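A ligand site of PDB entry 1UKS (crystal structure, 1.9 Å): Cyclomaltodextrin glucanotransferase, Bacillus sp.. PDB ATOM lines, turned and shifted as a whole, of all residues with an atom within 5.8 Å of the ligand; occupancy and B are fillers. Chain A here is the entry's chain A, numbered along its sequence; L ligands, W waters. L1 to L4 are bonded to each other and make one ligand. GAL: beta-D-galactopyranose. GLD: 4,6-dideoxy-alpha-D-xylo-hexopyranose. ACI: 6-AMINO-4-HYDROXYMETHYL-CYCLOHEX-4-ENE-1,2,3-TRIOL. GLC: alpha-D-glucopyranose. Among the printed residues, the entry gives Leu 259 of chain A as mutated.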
ATOM      1  N   ARG A  47      18.809 -17.226  15.590  1.00  0.00           N
ATOM      2  CA  ARG A  47      20.115 -17.716  15.155  1.00  0.00           C
ATOM      3  C   ARG A  47      20.048 -19.197  14.835  1.00  0.00           C
ATOM      4  O   ARG A  47      21.063 -19.850  14.534  1.00  0.00           O
ATOM      5  CB  ARG A  47      21.156 -17.481  16.247  1.00  0.00           C
ATOM      6  CG  ARG A  47      21.336 -16.009  16.541  1.00  0.00           C
ATOM      7  CD  ARG A  47      21.998 -15.892  17.891  1.00  0.00           C
ATOM      8  NE  ARG A  47      22.005 -14.549  18.444  1.00  0.00           N
ATOM      9  CZ  ARG A  47      22.824 -13.582  17.986  1.00  0.00           C
ATOM     10  NH1 ARG A  47      23.706 -13.764  16.992  1.00  0.00           N
ATOM     11  NH2 ARG A  47      22.778 -12.405  18.611  1.00  0.00           N
ATOM     12  N   TYR A  89      27.866 -19.437  21.353  1.00  0.00           N
ATOM     13  CA  TYR A  89      28.660 -18.255  21.607  1.00  0.00           C
ATOM     14  C   TYR A  89      28.067 -17.636  22.838  1.00  0.00           C
ATOM     15  O   TYR A  89      26.963 -17.093  22.803  1.00  0.00           O
ATOM     16  CB  TYR A  89      28.551 -17.257  20.473  1.00  0.00           C
ATOM     17  CG  TYR A  89      29.327 -17.690  19.243  1.00  0.00           C
ATOM     18  CD1 TYR A  89      28.638 -18.085  18.104  1.00  0.00           C
ATOM     19  CD2 TYR A  89      30.729 -17.639  19.265  1.00  0.00           C
ATOM     20  CE1 TYR A  89      29.336 -18.444  16.958  1.00  0.00           C
ATOM     21  CE2 TYR A  89      31.427 -17.998  18.129  1.00  0.00           C
ATOM     22  CZ  TYR A  89      30.718 -18.401  16.991  1.00  0.00           C
ATOM     23  OH  TYR A  89      31.413 -18.810  15.875  1.00  0.00           O
ATOM     24  N   VAL A  92      24.422 -18.312  23.755  1.00  0.00           N
ATOM     25  CA  VAL A  92      23.467 -18.542  22.690  1.00  0.00           C
ATOM     26  C   VAL A  92      24.032 -19.375  21.559  1.00  0.00           C
ATOM     27  O   VAL A  92      25.150 -19.208  21.095  1.00  0.00           O
ATOM     28  CB  VAL A  92      22.933 -17.128  22.238  1.00  0.00           C
ATOM     29  CG1 VAL A  92      24.049 -16.288  21.645  1.00  0.00           C
ATOM     30  CG2 VAL A  92      21.802 -17.318  21.231  1.00  0.00           C
ATOM     31  N   ASN A  94      24.166 -20.966  17.815  1.00  0.00           N
ATOM     32  CA  ASN A  94      24.201 -20.364  16.493  1.00  0.00           C
ATOM     33  C   ASN A  94      24.323 -21.465  15.473  1.00  0.00           C
ATOM     34  O   ASN A  94      24.993 -22.469  15.749  1.00  0.00           O
ATOM     35  CB  ASN A  94      25.386 -19.487  16.347  1.00  0.00           C
ATOM     36  CG  ASN A  94      25.256 -18.137  17.007  1.00  0.00           C
ATOM     37  OD1 ASN A  94      25.331 -17.111  16.325  1.00  0.00           O
ATOM     38  ND2 ASN A  94      25.125 -18.043  18.325  1.00  0.00           N
ATOM     39  N   TYR A  97      22.311 -20.958   9.385  1.00  0.00           N
ATOM     40  CA  TYR A  97      21.031 -20.675   8.697  1.00  0.00           C
ATOM     41  C   TYR A  97      21.177 -19.693   7.541  1.00  0.00           C
ATOM     42  O   TYR A  97      20.443 -19.730   6.545  1.00  0.00           O
ATOM     43  CB  TYR A  97      19.971 -20.127   9.721  1.00  0.00           C
ATOM     44  CG  TYR A  97      20.186 -18.668  10.144  1.00  0.00           C
ATOM     45  CD1 TYR A  97      19.618 -17.629   9.373  1.00  0.00           C
ATOM     46  CD2 TYR A  97      21.009 -18.358  11.206  1.00  0.00           C
ATOM     47  CE1 TYR A  97      19.882 -16.301   9.653  1.00  0.00           C
ATOM     48  CE2 TYR A  97      21.281 -17.023  11.506  1.00  0.00           C
ATOM     49  CZ  TYR A  97      20.713 -15.998  10.715  1.00  0.00           C
ATOM     50  OH  TYR A  97      21.004 -14.683  10.974  1.00  0.00           O
ATOM     51  N   HIS A  98      22.136 -18.786   7.726  1.00  0.00           N
ATOM     52  CA  HIS A  98      22.459 -17.712   6.782  1.00  0.00           C
ATOM     53  C   HIS A  98      23.282 -18.108   5.549  1.00  0.00           C
ATOM     54  O   HIS A  98      23.548 -17.263   4.687  1.00  0.00           O
ATOM     55  CB  HIS A  98      23.162 -16.628   7.571  1.00  0.00           C
ATOM     56  CG  HIS A  98      24.359 -17.143   8.382  1.00  0.00           C
ATOM     57  ND1 HIS A  98      25.463 -17.720   7.937  1.00  0.00           N
ATOM     58  CD2 HIS A  98      24.452 -17.102   9.750  1.00  0.00           C
ATOM     59  CE1 HIS A  98      26.230 -18.036   8.970  1.00  0.00           C
ATOM     60  NE2 HIS A  98      25.598 -17.659  10.043  1.00  0.00           N
ATOM     61  N   TYR A 100      26.490 -18.687   5.242  1.00  0.00           N
ATOM     62  CA  TYR A 100      27.810 -18.094   5.109  1.00  0.00           C
ATOM     63  C   TYR A 100      28.973 -18.913   5.651  1.00  0.00           C
ATOM     64  O   TYR A 100      30.109 -18.436   5.577  1.00  0.00           O
ATOM     65  CB  TYR A 100      27.902 -16.741   5.828  1.00  0.00           C
ATOM     66  CG  TYR A 100      26.995 -15.627   5.284  1.00  0.00           C
ATOM     67  CD1 TYR A 100      27.108 -15.177   3.968  1.00  0.00           C
ATOM     68  CD2 TYR A 100      26.085 -14.993   6.141  1.00  0.00           C
ATOM     69  CE1 TYR A 100      26.328 -14.107   3.528  1.00  0.00           C
ATOM     70  CE2 TYR A 100      25.291 -13.924   5.701  1.00  0.00           C
ATOM     71  CZ  TYR A 100      25.427 -13.480   4.394  1.00  0.00           C
ATOM     72  OH  TYR A 100      24.682 -12.401   3.952  1.00  0.00           O
ATOM     73  N   TRP A 101      28.736 -20.067   6.251  1.00  0.00           N
ATOM     74  CA  TRP A 101      29.788 -20.849   6.879  1.00  0.00           C
ATOM     75  C   TRP A 101      30.000 -22.131   6.075  1.00  0.00           C
ATOM     76  O   TRP A 101      29.647 -23.253   6.480  1.00  0.00           O
ATOM     77  CB  TRP A 101      29.361 -21.130   8.311  1.00  0.00           C
ATOM     78  CG  TRP A 101      29.290 -19.955   9.288  1.00  0.00           C
ATOM     79  CD1 TRP A 101      29.821 -18.705   9.025  1.00  0.00           C
ATOM     80  CD2 TRP A 101      28.729 -20.015  10.537  1.00  0.00           C
ATOM     81  NE1 TRP A 101      29.600 -17.998  10.118  1.00  0.00           N
ATOM     82  CE2 TRP A 101      28.963 -18.732  11.039  1.00  0.00           C
ATOM     83  CE3 TRP A 101      28.082 -20.962  11.327  1.00  0.00           C
ATOM     84  CZ2 TRP A 101      28.555 -18.374  12.321  1.00  0.00           C
ATOM     85  CZ3 TRP A 101      27.680 -20.596  12.609  1.00  0.00           C
ATOM     86  CH2 TRP A 101      27.907 -19.321  13.101  1.00  0.00           C
ATOM     87  N   HIS A 140      36.265 -17.219   3.038  1.00  0.00           N
ATOM     88  CA  HIS A 140      36.452 -18.016   4.229  1.00  0.00           C
ATOM     89  C   HIS A 140      35.627 -19.285   4.126  1.00  0.00           C
ATOM     90  O   HIS A 140      34.779 -19.363   3.226  1.00  0.00           O
ATOM     91  CB  HIS A 140      36.007 -17.206   5.473  1.00  0.00           C
ATOM     92  CG  HIS A 140      34.555 -16.672   5.425  1.00  0.00           C
ATOM     93  ND1 HIS A 140      34.073 -15.433   5.141  1.00  0.00           N
ATOM     94  CD2 HIS A 140      33.451 -17.488   5.547  1.00  0.00           C
ATOM     95  CE1 HIS A 140      32.762 -15.514   5.064  1.00  0.00           C
ATOM     96  NE2 HIS A 140      32.420 -16.749   5.308  1.00  0.00           N
ATOM     97  N   PRO A 143      33.573 -20.997  11.260  1.00  0.00           N
ATOM     98  CA  PRO A 143      34.263 -20.787  12.549  1.00  0.00           C
ATOM     99  C   PRO A 143      35.321 -21.886  12.845  1.00  0.00           C
ATOM    100  O   PRO A 143      35.080 -23.071  12.594  1.00  0.00           O
ATOM    101  CB  PRO A 143      33.102 -20.717  13.516  1.00  0.00           C
ATOM    102  CG  PRO A 143      32.025 -20.014  12.729  1.00  0.00           C
ATOM    103  CD  PRO A 143      32.139 -20.781  11.431  1.00  0.00           C
ATOM    104  N   LEU A 194      38.593 -12.456  10.013  1.00  0.00           N
ATOM    105  CA  LEU A 194      37.496 -11.652  10.519  1.00  0.00           C
ATOM    106  C   LEU A 194      36.653 -12.566  11.419  1.00  0.00           C
ATOM    107  O   LEU A 194      36.226 -13.667  11.047  1.00  0.00           O
ATOM    108  CB  LEU A 194      36.796 -11.163   9.273  1.00  0.00           C
ATOM    109  CG  LEU A 194      35.615 -10.226   9.212  1.00  0.00           C
ATOM    110  CD1 LEU A 194      35.911  -8.884   9.881  1.00  0.00           C
ATOM    111  CD2 LEU A 194      35.289 -10.100   7.726  1.00  0.00           C
ATOM    112  N   TYR A 195      36.429 -12.107  12.642  1.00  0.00           N
ATOM    113  CA  TYR A 195      35.713 -12.832  13.687  1.00  0.00           C
ATOM    114  C   TYR A 195      36.557 -14.103  13.943  1.00  0.00           C
ATOM    115  O   TYR A 195      37.769 -14.006  14.185  1.00  0.00           O
ATOM    116  CB  TYR A 195      34.257 -13.216  13.256  1.00  0.00           C
ATOM    117  CG  TYR A 195      33.363 -12.129  12.681  1.00  0.00           C
ATOM    118  CD1 TYR A 195      32.723 -11.200  13.515  1.00  0.00           C
ATOM    119  CD2 TYR A 195      33.167 -12.090  11.299  1.00  0.00           C
ATOM    120  CE1 TYR A 195      31.884 -10.231  12.937  1.00  0.00           C
ATOM    121  CE2 TYR A 195      32.336 -11.128  10.721  1.00  0.00           C
ATOM    122  CZ  TYR A 195      31.695 -10.198  11.545  1.00  0.00           C
ATOM    123  OH  TYR A 195      30.864  -9.236  10.967  1.00  0.00           O
ATOM    124  N   ASP A 196      35.998 -15.304  13.838  1.00  0.00           N
ATOM    125  CA  ASP A 196      36.712 -16.539  14.071  1.00  0.00           C
ATOM    126  C   ASP A 196      36.683 -17.391  12.809  1.00  0.00           C
ATOM    127  O   ASP A 196      36.835 -18.623  12.859  1.00  0.00           O
ATOM    128  CB  ASP A 196      36.022 -17.256  15.224  1.00  0.00           C
ATOM    129  CG  ASP A 196      34.522 -17.522  15.036  1.00  0.00           C
ATOM    130  OD1 ASP A 196      33.886 -16.982  14.127  1.00  0.00           O
ATOM    131  OD2 ASP A 196      34.002 -18.300  15.831  1.00  0.00           O
ATOM    132  N   LEU A 197      36.450 -16.767  11.660  1.00  0.00           N
ATOM    133  CA  LEU A 197      36.271 -17.535  10.446  1.00  0.00           C
ATOM    134  C   LEU A 197      37.607 -17.937   9.849  1.00  0.00           C
ATOM    135  O   LEU A 197      38.515 -17.116   9.777  1.00  0.00           O
ATOM    136  CB  LEU A 197      35.453 -16.669   9.466  1.00  0.00           C
ATOM    137  CG  LEU A 197      34.065 -16.226   9.915  1.00  0.00           C
ATOM    138  CD1 LEU A 197      33.489 -15.299   8.874  1.00  0.00           C
ATOM    139  CD2 LEU A 197      33.175 -17.436  10.126  1.00  0.00           C
ATOM    140  N   ARG A 227      26.301 -12.402  -6.079  1.00  0.00           N
ATOM    141  CA  ARG A 227      26.571 -11.325  -5.159  1.00  0.00           C
ATOM    142  C   ARG A 227      27.754 -11.826  -4.336  1.00  0.00           C
ATOM    143  O   ARG A 227      27.610 -12.799  -3.580  1.00  0.00           O
ATOM    144  CB  ARG A 227      25.378 -11.066  -4.239  1.00  0.00           C
ATOM    145  CG  ARG A 227      25.465  -9.784  -3.399  1.00  0.00           C
ATOM    146  CD  ARG A 227      26.459  -9.665  -2.236  1.00  0.00           C
ATOM    147  NE  ARG A 227      26.121 -10.627  -1.210  1.00  0.00           N
ATOM    148  CZ  ARG A 227      26.547 -10.542   0.051  1.00  0.00           C
ATOM    149  NH1 ARG A 227      27.344  -9.573   0.464  1.00  0.00           N
ATOM    150  NH2 ARG A 227      26.105 -11.402   0.941  1.00  0.00           N
ATOM    151  N   VAL A 228      28.925 -11.191  -4.432  1.00  0.00           N
ATOM    152  CA  VAL A 228      30.001 -11.690  -3.614  1.00  0.00           C
ATOM    153  C   VAL A 228      30.216 -10.871  -2.351  1.00  0.00           C
ATOM    154  O   VAL A 228      30.184  -9.648  -2.267  1.00  0.00           O
ATOM    155  CB  VAL A 228      31.349 -11.913  -4.541  1.00  0.00           C
ATOM    156  CG1 VAL A 228      31.254 -11.289  -5.887  1.00  0.00           C
ATOM    157  CG2 VAL A 228      32.591 -11.456  -3.769  1.00  0.00           C
ATOM    158  N   ASP A 229      30.339 -11.670  -1.308  1.00  0.00           N
ATOM    159  CA  ASP A 229      30.505 -11.222   0.057  1.00  0.00           C
ATOM    160  C   ASP A 229      31.918 -10.776   0.390  1.00  0.00           C
ATOM    161  O   ASP A 229      32.867 -11.403  -0.068  1.00  0.00           O
ATOM    162  CB  ASP A 229      30.099 -12.385   0.945  1.00  0.00           C
ATOM    163  CG  ASP A 229      30.298 -12.205   2.438  1.00  0.00           C
ATOM    164  OD1 ASP A 229      29.499 -11.494   3.019  1.00  0.00           O
ATOM    165  OD2 ASP A 229      31.230 -12.773   3.002  1.00  0.00           O
ATOM    166  N   ALA A 230      32.048  -9.762   1.267  1.00  0.00           N
ATOM    167  CA  ALA A 230      33.310  -9.238   1.787  1.00  0.00           C
ATOM    168  C   ALA A 230      34.391  -8.844   0.784  1.00  0.00           C
ATOM    169  O   ALA A 230      35.577  -9.130   0.996  1.00  0.00           O
ATOM    170  CB  ALA A 230      33.867 -10.272   2.779  1.00  0.00           C
ATOM    171  N   VAL A 231      34.021  -8.120  -0.298  1.00  0.00           N
ATOM    172  CA  VAL A 231      35.004  -7.745  -1.316  1.00  0.00           C
ATOM    173  C   VAL A 231      36.105  -6.818  -0.797  1.00  0.00           C
ATOM    174  O   VAL A 231      37.181  -6.794  -1.399  1.00  0.00           O
ATOM    175  CB  VAL A 231      34.344  -7.062  -2.564  1.00  0.00           C
ATOM    176  CG1 VAL A 231      33.455  -8.105  -3.194  1.00  0.00           C
ATOM    177  CG2 VAL A 231      33.523  -5.841  -2.261  1.00  0.00           C
ATOM    178  N   LYS A 232      35.977  -6.086   0.323  1.00  0.00           N
ATOM    179  CA  LYS A 232      37.138  -5.312   0.748  1.00  0.00           C
ATOM    180  C   LYS A 232      38.083  -6.150   1.602  1.00  0.00           C
ATOM    181  O   LYS A 232      39.063  -5.639   2.136  1.00  0.00           O
ATOM    182  CB  LYS A 232      36.721  -4.075   1.522  1.00  0.00           C
ATOM    183  CG  LYS A 232      36.070  -4.224   2.855  1.00  0.00           C
ATOM    184  CD  LYS A 232      35.818  -2.822   3.391  1.00  0.00           C
ATOM    185  CE  LYS A 232      37.063  -1.994   3.703  1.00  0.00           C
ATOM    186  NZ  LYS A 232      36.693  -0.776   4.404  1.00  0.00           N
ATOM    187  N   HIS A 233      37.762  -7.432   1.785  1.00  0.00           N
ATOM    188  CA  HIS A 233      38.572  -8.312   2.604  1.00  0.00           C
ATOM    189  C   HIS A 233      39.273  -9.429   1.807  1.00  0.00           C
ATOM    190  O   HIS A 233      39.778 -10.421   2.361  1.00  0.00           O
ATOM    191  CB  HIS A 233      37.667  -8.889   3.688  1.00  0.00           C
ATOM    192  CG  HIS A 233      37.158  -7.805   4.617  1.00  0.00           C
ATOM    193  ND1 HIS A 233      37.850  -6.956   5.376  1.00  0.00           N
ATOM    194  CD2 HIS A 233      35.834  -7.514   4.782  1.00  0.00           C
ATOM    195  CE1 HIS A 233      37.006  -6.176   5.969  1.00  0.00           C
ATOM    196  NE2 HIS A 233      35.793  -6.521   5.607  1.00  0.00           N
ATOM    197  N   GLU A 257      29.691  -6.480  -1.936  1.00  0.00           N
ATOM    198  CA  GLU A 257      29.325  -5.667  -0.815  1.00  0.00           C
ATOM    199  C   GLU A 257      30.584  -5.080  -0.164  1.00  0.00           C
ATOM    200  O   GLU A 257      31.444  -5.829   0.333  1.00  0.00           O
ATOM    201  CB  GLU A 257      28.563  -6.499   0.201  1.00  0.00           C
ATOM    202  CG  GLU A 257      28.179  -5.680   1.403  1.00  0.00           C
ATOM    203  CD  GLU A 257      27.348  -6.367   2.453  1.00  0.00           C
ATOM    204  OE1 GLU A 257      26.918  -5.655   3.337  1.00  0.00           O
ATOM    205  OE2 GLU A 257      27.111  -7.574   2.402  1.00  0.00           O
ATOM    206  N   TRP A 258      30.715  -3.765  -0.148  1.00  0.00           N
ATOM    207  CA  TRP A 258      31.790  -3.038   0.503  1.00  0.00           C
ATOM    208  C   TRP A 258      30.910  -2.056   1.268  1.00  0.00           C
ATOM    209  O   TRP A 258      30.288  -1.134   0.730  1.00  0.00           O
ATOM    210  CB  TRP A 258      32.635  -2.350  -0.558  1.00  0.00           C
ATOM    211  CG  TRP A 258      33.781  -1.478  -0.051  1.00  0.00           C
ATOM    212  CD1 TRP A 258      33.645  -0.555   0.958  1.00  0.00           C
ATOM    213  CD2 TRP A 258      35.054  -1.495  -0.564  1.00  0.00           C
ATOM    214  NE1 TRP A 258      34.829   0.023   1.072  1.00  0.00           N
ATOM    215  CE2 TRP A 258      35.703  -0.499   0.188  1.00  0.00           C
ATOM    216  CE3 TRP A 258      35.733  -2.210  -1.560  1.00  0.00           C
ATOM    217  CZ2 TRP A 258      37.053  -0.208  -0.048  1.00  0.00           C
ATOM    218  CZ3 TRP A 258      37.091  -1.912  -1.775  1.00  0.00           C
ATOM    219  CH2 TRP A 258      37.733  -0.923  -1.033  1.00  0.00           C
ATOM    220  N   LEU A 259      30.882  -2.219   2.581  1.00  0.00           N
ATOM    221  CA  LEU A 259      30.019  -1.399   3.405  1.00  0.00           C
ATOM    222  C   LEU A 259      30.544   0.026   3.623  1.00  0.00           C
ATOM    223  O   LEU A 259      31.752   0.230   3.735  1.00  0.00           O
ATOM    224  CB  LEU A 259      29.870  -2.169   4.713  1.00  0.00           C
ATOM    225  CG  LEU A 259      28.793  -1.770   5.687  1.00  0.00           C
ATOM    226  CD1 LEU A 259      28.055  -3.045   6.040  1.00  0.00           C
ATOM    227  CD2 LEU A 259      29.382  -0.998   6.871  1.00  0.00           C
ATOM    228  N   HIS A 327      20.257  -7.117   4.869  1.00  0.00           N
ATOM    229  CA  HIS A 327      20.704  -7.937   5.987  1.00  0.00           C
ATOM    230  C   HIS A 327      21.739  -7.298   6.909  1.00  0.00           C
ATOM    231  O   HIS A 327      21.986  -7.801   8.007  1.00  0.00           O
ATOM    232  CB  HIS A 327      21.215  -9.227   5.348  1.00  0.00           C
ATOM    233  CG  HIS A 327      22.383  -8.977   4.401  1.00  0.00           C
ATOM    234  ND1 HIS A 327      22.424  -8.333   3.229  1.00  0.00           N
ATOM    235  CD2 HIS A 327      23.671  -9.379   4.698  1.00  0.00           C
ATOM    236  CE1 HIS A 327      23.680  -8.316   2.838  1.00  0.00           C
ATOM    237  NE2 HIS A 327      24.404  -8.951   3.722  1.00  0.00           N
ATOM    238  N   ASP A 328      22.392  -6.190   6.519  1.00  0.00           N
ATOM    239  CA  ASP A 328      23.389  -5.574   7.363  1.00  0.00           C
ATOM    240  C   ASP A 328      23.014  -4.221   7.955  1.00  0.00           C
ATOM    241  O   ASP A 328      23.846  -3.470   8.437  1.00  0.00           O
ATOM    242  CB  ASP A 328      24.698  -5.460   6.559  1.00  0.00           C
ATOM    243  CG  ASP A 328      25.585  -6.715   6.543  1.00  0.00           C
ATOM    244  OD1 ASP A 328      25.397  -7.661   7.311  1.00  0.00           O
ATOM    245  OD2 ASP A 328      26.497  -6.740   5.748  1.00  0.00           O
ATOM    246  N   ASP A 371      21.312  -7.401  12.917  1.00  0.00           N
ATOM    247  CA  ASP A 371      21.495  -8.837  12.965  1.00  0.00           C
ATOM    248  C   ASP A 371      21.427  -9.405  14.388  1.00  0.00           C
ATOM    249  O   ASP A 371      22.177  -8.928  15.244  1.00  0.00           O
ATOM    250  CB  ASP A 371      22.851  -9.125  12.307  1.00  0.00           C
ATOM    251  CG  ASP A 371      23.318 -10.568  12.212  1.00  0.00           C
ATOM    252  OD1 ASP A 371      24.517 -10.774  12.053  1.00  0.00           O
ATOM    253  OD2 ASP A 371      22.505 -11.477  12.269  1.00  0.00           O
ATOM    254  N   ARG A 375      16.335 -10.268  10.409  1.00  0.00           N
ATOM    255  CA  ARG A 375      16.127 -11.477   9.646  1.00  0.00           C
ATOM    256  C   ARG A 375      15.019 -12.338  10.218  1.00  0.00           C
ATOM    257  O   ARG A 375      15.132 -13.565  10.200  1.00  0.00           O
ATOM    258  CB  ARG A 375      17.425 -12.309   9.601  1.00  0.00           C
ATOM    259  CG  ARG A 375      18.511 -11.682   8.768  1.00  0.00           C
ATOM    260  CD  ARG A 375      19.665 -11.129   9.565  1.00  0.00           C
ATOM    261  NE  ARG A 375      20.774 -12.033   9.489  1.00  0.00           N
ATOM    262  CZ  ARG A 375      22.041 -11.739   9.167  1.00  0.00           C
ATOM    263  NH1 ARG A 375      22.508 -10.541   8.837  1.00  0.00           N
ATOM    264  NH2 ARG A 375      22.900 -12.748   9.244  1.00  0.00           N
HETATM  265  C1  GAL L   1      32.215  -5.267   4.642  1.00  0.00           C
HETATM  266  C2  GAL L   1      32.360  -6.480   3.691  1.00  0.00           C
HETATM  267  C3  GAL L   1      30.856  -7.067   3.823  1.00  0.00           C
HETATM  268  C4  GAL L   1      30.750  -7.709   5.269  1.00  0.00           C
HETATM  269  C5  GAL L   1      31.130  -6.641   6.384  1.00  0.00           C
HETATM  270  C6  GAL L   1      31.392  -7.392   7.711  1.00  0.00           C
HETATM  271  O1  GAL L   1      33.127  -4.232   4.270  1.00  0.00           O
HETATM  272  O2  GAL L   1      32.954  -6.115   2.402  1.00  0.00           O
HETATM  273  O3  GAL L   1      30.523  -7.999   2.786  1.00  0.00           O
HETATM  274  O4  GAL L   1      29.410  -8.247   5.623  1.00  0.00           O
HETATM  275  O5  GAL L   1      32.364  -5.860   5.985  1.00  0.00           O
HETATM  276  O6  GAL L   1      32.365  -8.422   7.481  1.00  0.00           O
HETATM  277  C1  GLD L   2      29.166  -9.587   5.141  1.00  0.00           C
HETATM  278  C2  GLD L   2      27.720 -10.086   5.401  1.00  0.00           C
HETATM  279  C3  GLD L   2      27.537 -10.314   6.951  1.00  0.00           C
HETATM  280  C4  GLD L   2      28.453 -11.526   7.294  1.00  0.00           C
HETATM  281  C5  GLD L   2      29.951 -11.073   7.052  1.00  0.00           C
HETATM  282  C6  GLD L   2      30.959 -12.266   7.241  1.00  0.00           C
HETATM  283  O2  GLD L   2      26.788  -9.151   4.907  1.00  0.00           O
HETATM  284  O3  GLD L   2      26.173 -10.500   7.427  1.00  0.00           O
HETATM  285  O5  GLD L   2      30.152 -10.584   5.672  1.00  0.00           O
HETATM  286  C1  ACI L   3      27.949 -13.475   8.917  1.00  0.00           C
HETATM  287  C2  ACI L   3      26.668 -13.666   9.789  1.00  0.00           C
HETATM  288  C3  ACI L   3      26.921 -13.533  11.319  1.00  0.00           C
HETATM  289  C4  ACI L   3      28.158 -14.299  11.838  1.00  0.00           C
HETATM  290  C5  ACI L   3      29.355 -14.402  10.849  1.00  0.00           C
HETATM  291  C6  ACI L   3      30.772 -14.615  11.370  1.00  0.00           C
HETATM  292  C7  ACI L   3      29.213 -14.155   9.474  1.00  0.00           C
HETATM  293  N1  ACI L   3      28.145 -12.014   8.660  1.00  0.00           N
HETATM  294  O2  ACI L   3      25.717 -12.625   9.447  1.00  0.00           O
HETATM  295  O3  ACI L   3      25.781 -14.091  11.984  1.00  0.00           O
HETATM  296  O4  ACI L   3      28.704 -13.649  13.045  1.00  0.00           O
HETATM  297  O6  ACI L   3      30.829 -16.008  11.655  1.00  0.00           O
HETATM  298  C1  GLC L   4      29.236 -14.592  14.058  1.00  0.00           C
HETATM  299  C2  GLC L   4      28.124 -15.065  15.082  1.00  0.00           C
HETATM  300  C3  GLC L   4      28.077 -14.146  16.298  1.00  0.00           C
HETATM  301  C4  GLC L   4      29.503 -14.132  16.929  1.00  0.00           C
HETATM  302  C5  GLC L   4      30.485 -13.417  15.942  1.00  0.00           C
HETATM  303  C6  GLC L   4      31.943 -13.486  16.572  1.00  0.00           C
HETATM  304  O2  GLC L   4      26.800 -15.075  14.506  1.00  0.00           O
HETATM  305  O3  GLC L   4      27.058 -14.600  17.227  1.00  0.00           O
HETATM  306  O4  GLC L   4      29.449 -13.460  18.215  1.00  0.00           O
HETATM  307  O5  GLC L   4      30.518 -14.124  14.647  1.00  0.00           O
HETATM  308  O6  GLC L   4      32.472 -14.813  16.413  1.00  0.00           O
HETATM  309  O   HOH W   1      33.703  -1.038   5.189  1.00  0.00           O
HETATM  310  O   HOH W   2      25.633 -14.663  19.629  1.00  0.00           O
HETATM  311  O   HOH W   3      31.308 -16.910  14.072  1.00  0.00           O
HETATM  312  O   HOH W   4      22.935 -14.036  12.833  1.00  0.00           O
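OD2 of Asp 328 is in hydrogen-bond range of O2 of GLD L2 (2.6 Å).
An oxygen (O2) of GAL L1 is in hydrogen-bond range of the backbone carbonyl oxygen (O) of Glu 257 (2.6 Å).
O2 of GLD L2 is in hydrogen-bond range of OE2 of Glu 257 (3.0 Å).
An oxygen (O2) of GLD L2 sits at hydrogen-bond distance from a ring nitrogen (NE2) of His 327, at 2.7 Å.
The backbone NH (N) of Ala 230 lies within hydrogen-bond range of an oxygen (O3) of GAL L1 (2.8 Å).
The indole nitrogen of Trp 101 sits at hydrogen-bond distance from an oxygen (O6) of ACI L3 (2.8 Å).
The guanidinium group (NH2) of Arg 375 lies within hydrogen-bond range of an oxygen (O2) of ACI L3 (2.8 Å).
An oxygen (O2) of GLC L4 lies within hydrogen-bond range of the side-chain amide oxygen (OD1) of Asn 94, 3.1 Å away.
The side-chain carboxylate (OD1) of Asp 371 sits at hydrogen-bond distance from an oxygen (O2) of ACI L3, 3.4 Å away.
The side-chain carboxylate of Asp 196 lies within hydrogen-bond range of an oxygen (O6) of GLC L4, 3.5 Å away.
N of Leu 259 lies within hydrogen-bond range of O1 of GAL L1 (3.5 Å).
NH1 of Arg 47 sits at hydrogen-bond distance from O3 of GLC L4 (3.5 Å).
OE1 of Glu 257 sits close to OD2 of Asp 328 (2.7 Å).
A ring nitrogen (NE2) of His 327 is in hydrogen-bond range of the side-chain carboxylate of Glu 257 (3.3 Å).
OE2 of Glu 257 is in salt-bridge range of NH1 of Arg 227 (2.8 Å).
O of Val 228 is in hydrogen-bond range of N of Glu 257 (3.2 Å).
The side-chain hydroxyl (OH) of Tyr 97 lies within hydrogen-bond range of the guanidinium group (NE) of Arg 375 (3.0 Å).
ND2 of Asn 94 is in hydrogen-bond range of O of Val 92 (3.0 Å).
A ring nitrogen (ND1) of His 98 lies within hydrogen-bond range of the backbone NH (N) of Tyr 100 (3.0 Å).
The guanidinium group of Arg 227 lies within hydrogen-bond range of the side-chain hydroxyl of Tyr 100, 3.5 Å away.
O5 of GLD L2 sits close to OD1 of Asp 229.
Residues that only touch the ligand: Leu 197, Lys 232, Leu 194, Tyr 195, His 233, Val 231, Tyr 100, Tyr 89, Trp 258 and His 98.
Within 4 Å of the ligand: Arg 47, Tyr 89, Asn 94, His 98, Tyr 100, Trp 101, Leu 194, Tyr 195, Asp 196, Leu 197, Asp 229, Ala 230, Val 231, Lys 232, His 233, Glu 257, Trp 258, Leu 259, His 327, Asp 328, Asp 371 and Arg 375.
Water W3 lies within hydrogen-bond range of the side-chain carboxylate (OD1) of Asp 196 (2.6 Å), the side-chain hydroxyl (OH) of Tyr 89 (2.6 Å) and an oxygen (O6) of ACI L3 (2.6 Å).
Water W2 lies within hydrogen-bond range of O3 of GLC L4 and NH1 of Arg 47.
Water W4 lies within hydrogen-bond range of the side-chain carboxylate (OD2) of Asp 371 (2.7 Å), the side-chain hydroxyl (OH) of Tyr 97 (2.8 Å) and an oxygen (O3) of ACI L3 (3.0 Å).
Water W1 lies within hydrogen-bond range of O of Leu 259 (2.7 Å), NZ of Lys 232 (3.1 Å) and O1 of GAL L1 (3.4 Å).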
